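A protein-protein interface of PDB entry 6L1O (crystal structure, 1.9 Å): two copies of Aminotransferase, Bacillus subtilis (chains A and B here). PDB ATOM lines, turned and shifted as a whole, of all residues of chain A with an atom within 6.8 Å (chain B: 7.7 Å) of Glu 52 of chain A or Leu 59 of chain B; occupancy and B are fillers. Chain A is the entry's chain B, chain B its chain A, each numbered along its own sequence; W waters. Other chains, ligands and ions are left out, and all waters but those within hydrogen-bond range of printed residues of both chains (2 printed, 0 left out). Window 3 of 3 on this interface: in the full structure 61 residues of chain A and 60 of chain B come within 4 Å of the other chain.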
ATOM      1  N   PRO A  47      18.142  27.851 -21.435  1.00  0.00           N
ATOM      2  CA  PRO A  47      17.904  29.255 -21.091  1.00  0.00           C
ATOM      3  C   PRO A  47      18.865  30.180 -21.790  1.00  0.00           C
ATOM      4  O   PRO A  47      20.095  29.862 -21.910  1.00  0.00           O
ATOM      5  CB  PRO A  47      18.093  29.301 -19.577  1.00  0.00           C
ATOM      6  CG  PRO A  47      17.798  27.915 -19.151  1.00  0.00           C
ATOM      7  CD  PRO A  47      18.174  27.000 -20.253  1.00  0.00           C
ATOM      8  N   PRO A  48      18.353  31.313 -22.292  1.00  0.00           N
ATOM      9  CA  PRO A  48      19.166  32.084 -23.189  1.00  0.00           C
ATOM     10  C   PRO A  48      20.412  32.677 -22.534  1.00  0.00           C
ATOM     11  O   PRO A  48      21.355  32.956 -23.257  1.00  0.00           O
ATOM     12  CB  PRO A  48      18.218  33.171 -23.724  1.00  0.00           C
ATOM     13  CG  PRO A  48      17.124  33.238 -22.758  1.00  0.00           C
ATOM     14  CD  PRO A  48      16.968  31.827 -22.222  1.00  0.00           C
ATOM     15  N   HIS A  49      20.441  32.835 -21.205  1.00  0.00           N
ATOM     16  CA  HIS A  49      21.660  33.396 -20.605  1.00  0.00           C
ATOM     17  C   HIS A  49      22.850  32.410 -20.702  1.00  0.00           C
ATOM     18  O   HIS A  49      24.018  32.806 -20.767  1.00  0.00           O
ATOM     19  CB  HIS A  49      21.438  33.880 -19.136  1.00  0.00           C
ATOM     20  CG  HIS A  49      21.253  32.788 -18.134  1.00  0.00           C
ATOM     21  ND1 HIS A  49      20.099  32.026 -18.049  1.00  0.00           N
ATOM     22  CD2 HIS A  49      22.084  32.311 -17.182  1.00  0.00           C
ATOM     23  CE1 HIS A  49      20.237  31.129 -17.085  1.00  0.00           C
ATOM     24  NE2 HIS A  49      21.432  31.281 -16.557  1.00  0.00           N
ATOM     25  N   ILE A  50      22.527  31.127 -20.674  1.00  0.00           N
ATOM     26  CA  ILE A  50      23.507  30.059 -20.822  1.00  0.00           C
ATOM     27  C   ILE A  50      24.059  30.037 -22.231  1.00  0.00           C
ATOM     28  O   ILE A  50      25.296  30.019 -22.445  1.00  0.00           O
ATOM     29  CB  ILE A  50      22.871  28.704 -20.412  1.00  0.00           C
ATOM     30  CG1 ILE A  50      22.398  28.773 -18.939  1.00  0.00           C
ATOM     31  CG2 ILE A  50      23.824  27.559 -20.669  1.00  0.00           C
ATOM     32  CD1 ILE A  50      21.553  27.587 -18.541  1.00  0.00           C
ATOM     33  N   VAL A  51      23.169  30.130 -23.207  1.00  0.00           N
ATOM     34  CA  VAL A  51      23.577  30.222 -24.600  1.00  0.00           C
ATOM     35  C   VAL A  51      24.467  31.449 -24.872  1.00  0.00           C
ATOM     36  O   VAL A  51      25.502  31.360 -25.586  1.00  0.00           O
ATOM     37  CB  VAL A  51      22.360  30.270 -25.539  1.00  0.00           C
ATOM     38  CG1 VAL A  51      22.786  30.558 -26.951  1.00  0.00           C
ATOM     39  CG2 VAL A  51      21.530  28.990 -25.426  1.00  0.00           C
ATOM     40  N   GLU A  52      24.065  32.584 -24.331  1.00  0.00           N
ATOM     41  CA  GLU A  52      24.855  33.806 -24.496  1.00  0.00           C
ATOM     42  C   GLU A  52      26.220  33.734 -23.794  1.00  0.00           C
ATOM     43  O   GLU A  52      27.207  34.298 -24.293  1.00  0.00           O
ATOM     44  CB  GLU A  52      24.076  35.003 -23.985  1.00  0.00           C
ATOM     45  CG  GLU A  52      22.941  35.423 -24.922  1.00  0.00           C
ATOM     46  CD  GLU A  52      23.308  35.496 -26.409  1.00  0.00           C
ATOM     47  OE1 GLU A  52      24.410  35.980 -26.726  1.00  0.00           O
ATOM     48  OE2 GLU A  52      22.496  35.062 -27.289  1.00  0.00           O
ATOM     49  N   ALA A  53      26.280  33.042 -22.671  1.00  0.00           N
ATOM     50  CA  ALA A  53      27.585  32.825 -22.018  1.00  0.00           C
ATOM     51  C   ALA A  53      28.531  32.016 -22.934  1.00  0.00           C
ATOM     52  O   ALA A  53      29.684  32.367 -23.084  1.00  0.00           O
ATOM     53  CB  ALA A  53      27.408  32.125 -20.696  1.00  0.00           C
ATOM     54  N   LEU A  54      28.037  30.934 -23.554  1.00  0.00           N
ATOM     55  CA  LEU A  54      28.786  30.194 -24.560  1.00  0.00           C
ATOM     56  C   LEU A  54      29.252  31.106 -25.705  1.00  0.00           C
ATOM     57  O   LEU A  54      30.426  31.110 -26.099  1.00  0.00           O
ATOM     58  CB  LEU A  54      27.985  28.992 -25.119  1.00  0.00           C
ATOM     59  CG  LEU A  54      28.618  28.205 -26.269  1.00  0.00           C
ATOM     60  CD1 LEU A  54      30.007  27.709 -25.960  1.00  0.00           C
ATOM     61  CD2 LEU A  54      27.772  27.040 -26.740  1.00  0.00           C
ATOM     62  N   ARG A  55      28.339  31.921 -26.214  1.00  0.00           N
ATOM     63  CA  ARG A  55      28.647  32.731 -27.390  1.00  0.00           C
ATOM     64  C   ARG A  55      29.730  33.745 -27.084  1.00  0.00           C
ATOM     65  O   ARG A  55      30.624  33.896 -27.851  1.00  0.00           O
ATOM     66  CB  ARG A  55      27.415  33.410 -27.963  1.00  0.00           C
ATOM     67  CG  ARG A  55      26.450  32.385 -28.540  1.00  0.00           C
ATOM     68  CD  ARG A  55      25.130  32.987 -28.893  1.00  0.00           C
ATOM     69  NE  ARG A  55      25.232  33.578 -30.220  1.00  0.00           N
ATOM     70  CZ  ARG A  55      25.340  34.873 -30.475  1.00  0.00           C
ATOM     71  NH1 ARG A  55      25.368  35.745 -29.505  1.00  0.00           N
ATOM     72  NH2 ARG A  55      25.447  35.276 -31.715  1.00  0.00           N
ATOM     73  N   GLU A  56      29.664  34.369 -25.909  1.00  0.00           N
ATOM     74  CA  GLU A  56      30.673  35.337 -25.522  1.00  0.00           C
ATOM     75  C   GLU A  56      32.005  34.630 -25.231  1.00  0.00           C
ATOM     76  O   GLU A  56      33.046  35.052 -25.719  1.00  0.00           O
ATOM     77  CB  GLU A  56      30.257  36.102 -24.273  1.00  0.00           C
ATOM     78  N   ALA A  57      31.961  33.551 -24.452  1.00  0.00           N
ATOM     79  CA  ALA A  57      33.145  32.772 -24.124  1.00  0.00           C
ATOM     80  C   ALA A  57      33.934  32.280 -25.332  1.00  0.00           C
ATOM     81  O   ALA A  57      35.163  32.220 -25.316  1.00  0.00           O
ATOM     82  CB  ALA A  57      32.741  31.582 -23.253  1.00  0.00           C
ATOM     83  N   TRP A 246      24.405  19.294 -24.760  1.00  0.00           N
ATOM     84  CA  TRP A 246      25.678  19.979 -24.449  1.00  0.00           C
ATOM     85  C   TRP A 246      26.751  19.017 -23.881  1.00  0.00           C
ATOM     86  O   TRP A 246      27.959  19.283 -23.985  1.00  0.00           O
ATOM     87  CB  TRP A 246      25.424  21.112 -23.457  1.00  0.00           C
ATOM     88  CG  TRP A 246      24.560  22.258 -23.955  1.00  0.00           C
ATOM     89  CD1 TRP A 246      23.272  22.198 -24.460  1.00  0.00           C
ATOM     90  CD2 TRP A 246      24.944  23.638 -24.020  1.00  0.00           C
ATOM     91  NE1 TRP A 246      22.828  23.469 -24.775  1.00  0.00           N
ATOM     92  CE2 TRP A 246      23.839  24.366 -24.517  1.00  0.00           C
ATOM     93  CE3 TRP A 246      26.106  24.339 -23.654  1.00  0.00           C
ATOM     94  CZ2 TRP A 246      23.878  25.744 -24.690  1.00  0.00           C
ATOM     95  CZ3 TRP A 246      26.122  25.735 -23.834  1.00  0.00           C
ATOM     96  CH2 TRP A 246      25.028  26.405 -24.371  1.00  0.00           C
ATOM     97  N   GLN A 278      32.343  27.807 -19.284  1.00  0.00           N
ATOM     98  CA  GLN A 278      31.819  29.085 -18.895  1.00  0.00           C
ATOM     99  C   GLN A 278      30.277  29.094 -18.931  1.00  0.00           C
ATOM    100  O   GLN A 278      29.664  29.678 -18.070  1.00  0.00           O
ATOM    101  CB  GLN A 278      32.357  30.193 -19.749  1.00  0.00           C
ATOM    102  CG  GLN A 278      32.042  31.586 -19.216  1.00  0.00           C
ATOM    103  CD  GLN A 278      32.933  32.625 -19.824  1.00  0.00           C
ATOM    104  OE1 GLN A 278      34.125  32.405 -19.924  1.00  0.00           O
ATOM    105  NE2 GLN A 278      32.363  33.737 -20.278  1.00  0.00           N
ATOM    106  N   ALA B  53      30.692  30.232 -36.609  1.00  0.00           N
ATOM    107  CA  ALA B  53      29.822  29.091 -36.872  1.00  0.00           C
ATOM    108  C   ALA B  53      29.340  28.440 -35.553  1.00  0.00           C
ATOM    109  O   ALA B  53      28.152  28.092 -35.432  1.00  0.00           O
ATOM    110  CB  ALA B  53      30.507  28.099 -37.791  1.00  0.00           C
ATOM    111  N   LEU B  54      30.213  28.331 -34.542  1.00  0.00           N
ATOM    112  CA  LEU B  54      29.789  27.933 -33.232  1.00  0.00           C
ATOM    113  C   LEU B  54      28.737  28.872 -32.640  1.00  0.00           C
ATOM    114  O   LEU B  54      27.686  28.414 -32.153  1.00  0.00           O
ATOM    115  CB  LEU B  54      30.945  27.796 -32.243  1.00  0.00           C
ATOM    116  CG  LEU B  54      30.598  27.482 -30.783  1.00  0.00           C
ATOM    117  CD1 LEU B  54      29.898  26.139 -30.599  1.00  0.00           C
ATOM    118  CD2 LEU B  54      31.858  27.531 -29.893  1.00  0.00           C
ATOM    119  N   ARG B  55      29.000  30.192 -32.715  1.00  0.00           N
ATOM    120  CA  ARG B  55      28.138  31.152 -32.097  1.00  0.00           C
ATOM    121  C   ARG B  55      26.720  31.119 -32.722  1.00  0.00           C
ATOM    122  O   ARG B  55      25.763  31.187 -31.978  1.00  0.00           O
ATOM    123  CB  ARG B  55      28.733  32.543 -32.201  1.00  0.00           C
ATOM    124  CG  ARG B  55      29.856  32.746 -31.228  1.00  0.00           C
ATOM    125  CD  ARG B  55      30.679  33.971 -31.568  1.00  0.00           C
ATOM    126  NE  ARG B  55      29.849  35.090 -31.994  1.00  0.00           N
ATOM    127  CZ  ARG B  55      29.272  35.936 -31.182  1.00  0.00           C
ATOM    128  NH1 ARG B  55      29.458  35.826 -29.877  1.00  0.00           N
ATOM    129  NH2 ARG B  55      28.540  36.900 -31.676  1.00  0.00           N
ATOM    130  N   GLU B  56      26.633  30.966 -34.038  1.00  0.00           N
ATOM    131  CA  GLU B  56      25.370  30.861 -34.758  1.00  0.00           C
ATOM    132  C   GLU B  56      24.639  29.559 -34.452  1.00  0.00           C
ATOM    133  O   GLU B  56      23.430  29.547 -34.240  1.00  0.00           O
ATOM    134  CB  GLU B  56      25.598  30.990 -36.259  1.00  0.00           C
ATOM    135  CG  GLU B  56      24.340  31.044 -37.096  1.00  0.00           C
ATOM    136  CD  GLU B  56      23.479  32.326 -36.883  1.00  0.00           C
ATOM    137  OE1 GLU B  56      23.959  33.302 -36.269  1.00  0.00           O
ATOM    138  OE2 GLU B  56      22.291  32.361 -37.313  1.00  0.00           O
ATOM    139  N   ALA B  57      25.384  28.471 -34.423  1.00  0.00           N
ATOM    140  CA  ALA B  57      24.819  27.139 -34.188  1.00  0.00           C
ATOM    141  C   ALA B  57      24.225  27.010 -32.830  1.00  0.00           C
ATOM    142  O   ALA B  57      23.207  26.340 -32.638  1.00  0.00           O
ATOM    143  CB  ALA B  57      25.902  26.122 -34.369  1.00  0.00           C
ATOM    144  N   SER B  58      24.837  27.675 -31.843  1.00  0.00           N
ATOM    145  CA  SER B  58      24.396  27.545 -30.497  1.00  0.00           C
ATOM    146  C   SER B  58      22.990  28.122 -30.273  1.00  0.00           C
ATOM    147  O   SER B  58      22.371  27.810 -29.302  1.00  0.00           O
ATOM    148  CB  SER B  58      25.433  28.155 -29.540  1.00  0.00           C
ATOM    149  OG  SER B  58      25.241  29.573 -29.445  1.00  0.00           O
ATOM    150  N   LEU B  59      22.519  28.958 -31.196  1.00  0.00           N
ATOM    151  CA  LEU B  59      21.178  29.583 -31.085  1.00  0.00           C
ATOM    152  C   LEU B  59      20.086  28.625 -31.544  1.00  0.00           C
ATOM    153  O   LEU B  59      18.910  28.878 -31.301  1.00  0.00           O
ATOM    154  CB  LEU B  59      21.089  30.848 -31.901  1.00  0.00           C
ATOM    155  CG  LEU B  59      21.997  32.015 -31.524  1.00  0.00           C
ATOM    156  CD1 LEU B  59      21.975  33.020 -32.656  1.00  0.00           C
ATOM    157  CD2 LEU B  59      21.545  32.640 -30.241  1.00  0.00           C
ATOM    158  N   ASN B  60      20.484  27.535 -32.185  1.00  0.00           N
ATOM    159  CA  ASN B  60      19.554  26.569 -32.720  1.00  0.00           C
ATOM    160  C   ASN B  60      19.114  25.584 -31.619  1.00  0.00           C
ATOM    161  O   ASN B  60      19.899  24.742 -31.195  1.00  0.00           O
ATOM    162  CB  ASN B  60      20.165  25.858 -33.891  1.00  0.00           C
ATOM    163  CG  ASN B  60      19.234  24.879 -34.549  1.00  0.00           C
ATOM    164  OD1 ASN B  60      18.100  24.629 -34.090  1.00  0.00           O
ATOM    165  ND2 ASN B  60      19.722  24.274 -35.598  1.00  0.00           N
ATOM    166  N   PRO B  61      17.867  25.685 -31.188  1.00  0.00           N
ATOM    167  CA  PRO B  61      17.382  24.814 -30.117  1.00  0.00           C
ATOM    168  C   PRO B  61      17.357  23.332 -30.435  1.00  0.00           C
ATOM    169  O   PRO B  61      17.331  22.521 -29.506  1.00  0.00           O
ATOM    170  CB  PRO B  61      16.001  25.384 -29.779  1.00  0.00           C
ATOM    171  CG  PRO B  61      15.588  26.187 -30.942  1.00  0.00           C
ATOM    172  CD  PRO B  61      16.827  26.649 -31.633  1.00  0.00           C
ATOM    173  N   SER B  62      17.421  22.955 -31.727  1.00  0.00           N
ATOM    174  CA  SER B  62      17.610  21.578 -32.092  1.00  0.00           C
ATOM    175  C   SER B  62      18.851  20.979 -31.503  1.00  0.00           C
ATOM    176  O   SER B  62      18.922  19.768 -31.251  1.00  0.00           O
ATOM    177  CB  SER B  62      17.678  21.406 -33.605  1.00  0.00           C
ATOM    178  OG  SER B  62      16.411  21.623 -34.169  1.00  0.00           O
ATOM    179  N   PHE B  63      19.887  21.791 -31.283  1.00  0.00           N
ATOM    180  CA  PHE B  63      21.111  21.268 -30.646  1.00  0.00           C
ATOM    181  C   PHE B  63      21.099  21.306 -29.129  1.00  0.00           C
ATOM    182  O   PHE B  63      22.025  20.844 -28.480  1.00  0.00           O
ATOM    183  CB  PHE B  63      22.316  22.107 -31.154  1.00  0.00           C
ATOM    184  CG  PHE B  63      22.571  21.966 -32.623  1.00  0.00           C
ATOM    185  CD1 PHE B  63      22.427  20.761 -33.259  1.00  0.00           C
ATOM    186  CD2 PHE B  63      23.051  23.054 -33.360  1.00  0.00           C
ATOM    187  CE1 PHE B  63      22.719  20.628 -34.611  1.00  0.00           C
ATOM    188  CE2 PHE B  63      23.339  22.927 -34.725  1.00  0.00           C
ATOM    189  CZ  PHE B  63      23.164  21.713 -35.359  1.00  0.00           C
ATOM    190  N   HIS B  64      20.082  21.899 -28.515  1.00  0.00           N
ATOM    191  CA  HIS B  64      19.992  21.909 -27.067  1.00  0.00           C
ATOM    192  C   HIS B  64      19.690  20.556 -26.469  1.00  0.00           C
ATOM    193  O   HIS B  64      20.130  20.266 -25.358  1.00  0.00           O
ATOM    194  CB  HIS B  64      18.987  22.948 -26.594  1.00  0.00           C
ATOM    195  CG  HIS B  64      19.344  24.350 -27.007  1.00  0.00           C
ATOM    196  ND1 HIS B  64      18.583  25.436 -26.664  1.00  0.00           N
ATOM    197  CD2 HIS B  64      20.354  24.833 -27.742  1.00  0.00           C
ATOM    198  CE1 HIS B  64      19.117  26.527 -27.170  1.00  0.00           C
ATOM    199  NE2 HIS B  64      20.171  26.176 -27.858  1.00  0.00           N
ATOM    200  N   PHE B 273      28.058  18.210 -28.652  1.00  0.00           N
ATOM    201  CA  PHE B 273      27.261  19.398 -28.874  1.00  0.00           C
ATOM    202  C   PHE B 273      27.210  19.756 -30.340  1.00  0.00           C
ATOM    203  O   PHE B 273      28.234  19.865 -31.006  1.00  0.00           O
ATOM    204  CB  PHE B 273      27.757  20.568 -28.025  1.00  0.00           C
ATOM    205  CG  PHE B 273      26.904  21.805 -28.103  1.00  0.00           C
ATOM    206  CD1 PHE B 273      25.573  21.764 -27.737  1.00  0.00           C
ATOM    207  CD2 PHE B 273      27.438  23.035 -28.505  1.00  0.00           C
ATOM    208  CE1 PHE B 273      24.789  22.904 -27.780  1.00  0.00           C
ATOM    209  CE2 PHE B 273      26.658  24.172 -28.518  1.00  0.00           C
ATOM    210  CZ  PHE B 273      25.324  24.088 -28.192  1.00  0.00           C
ATOM    211  N   GLY B 275      26.565  22.440 -31.763  1.00  0.00           N
ATOM    212  CA  GLY B 275      27.216  23.721 -32.024  1.00  0.00           C
ATOM    213  C   GLY B 275      28.668  23.482 -32.389  1.00  0.00           C
ATOM    214  O   GLY B 275      29.182  24.080 -33.320  1.00  0.00           O
HETATM  215  O   HOH W   1      25.736  34.280 -34.237  1.00  0.00           O
HETATM  216  O   HOH W   2      29.700  18.329 -26.248  1.00  0.00           O
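Arg 55 of chain B touches its own counterpart, Arg 55 of chain A.
Positions printed for both chains: 53, 54, 55, 56 and 57.
Of the 10 pairs that touch across the chains among the printed residues, 1 has its exchanged pair printed and touching as well.
Ser 58 of chain B touches Val 51 of chain A.
His 64 of chain B touches Val 51 of chain A.
Glu 52 of chain A touches Leu 59 of chain B (OE2 to CD2, 3.9 Å).
Leu 54 of chain A touches Ser 58 of chain B.
Leu 54 of chain A touches Phe 273 of chain B (CD2 to CE2, 3.6 Å).
Arg 55 of chain A touches Ser 58 of chain B.
Arg 55 of chain A touches Leu 59 of chain B.
CD1 of Trp 246 of chain A touches O of His 64 of chain B, 3.8 Å away.
Trp 246 of chain A touches Phe 273 of chain B (NE1 to CE1, 3.6 Å).
OG of Ser 58 of chain B sits at hydrogen-bond distance from O of Arg 55 of chain B, at 3.0 Å.
The backbone carbonyl oxygen (O) of Ser 58 of chain B sits at hydrogen-bond distance from a ring nitrogen (NE2) of His 64 of chain B (3.1 Å).
The guanidinium group of Arg 55 of chain A is in salt-bridge range of the side-chain carboxylate of Glu 52 of chain A (2.9 Å).
Printed residues of chain A that touch a printed residue of chain B: Val 51, Glu 52, Leu 54, Arg 55 and Trp 246.
Hydrophobic or aromatic side chains of chain A that line the printed part of chain B: Val 51, Leu 54 and Trp 246.
Of the 14 printed residues of chain B, 5 touch a printed residue of chain A.
Among the printed residues, no Asp or Glu carboxylate lies within 4 Å of a Lys or Arg side-chain nitrogen of the other chain.
Of chain B, only Leu 59 comes within 4 Å of Glu 52 of chain A.
Ala 53 of chain A touches none of the printed residues of chain B.
Of the printed residues of chain A, Arg 55 of chain B touches Arg 55 (3.0 Å).
Of the printed residues of chain A, Ser 58 of chain B touches Val 51 (3.6 Å), Leu 54 (3.8 Å) and Arg 55 (3.2 Å).
Gly 275 of chain B touches none of the printed residues of chain A.
The nearest residue of chain B that does not touch Glu 52 of chain A is Arg 55 of chain B (6.0 Å).
The nearest printed residue of chain B that does not touch Trp 246 of chain A is Phe 63 of chain B (4.4 Å).
NE of Arg 55 of chain A lies within hydrogen-bond range of O of Arg 55 of chain B, 3.0 Å away.
Water W1 lies within hydrogen-bond range of the guanidinium group (NH2) of Arg 55 of chain A (2.7 Å) and the side-chain carboxylate (OE1) of Glu 56 of chain B (2.9 Å).
Water W2 bridges the backbone NH of Phe 273 of chain B (2.9 Å) and the backbone carbonyl oxygen of Trp 246 of chain A (3.0 Å).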
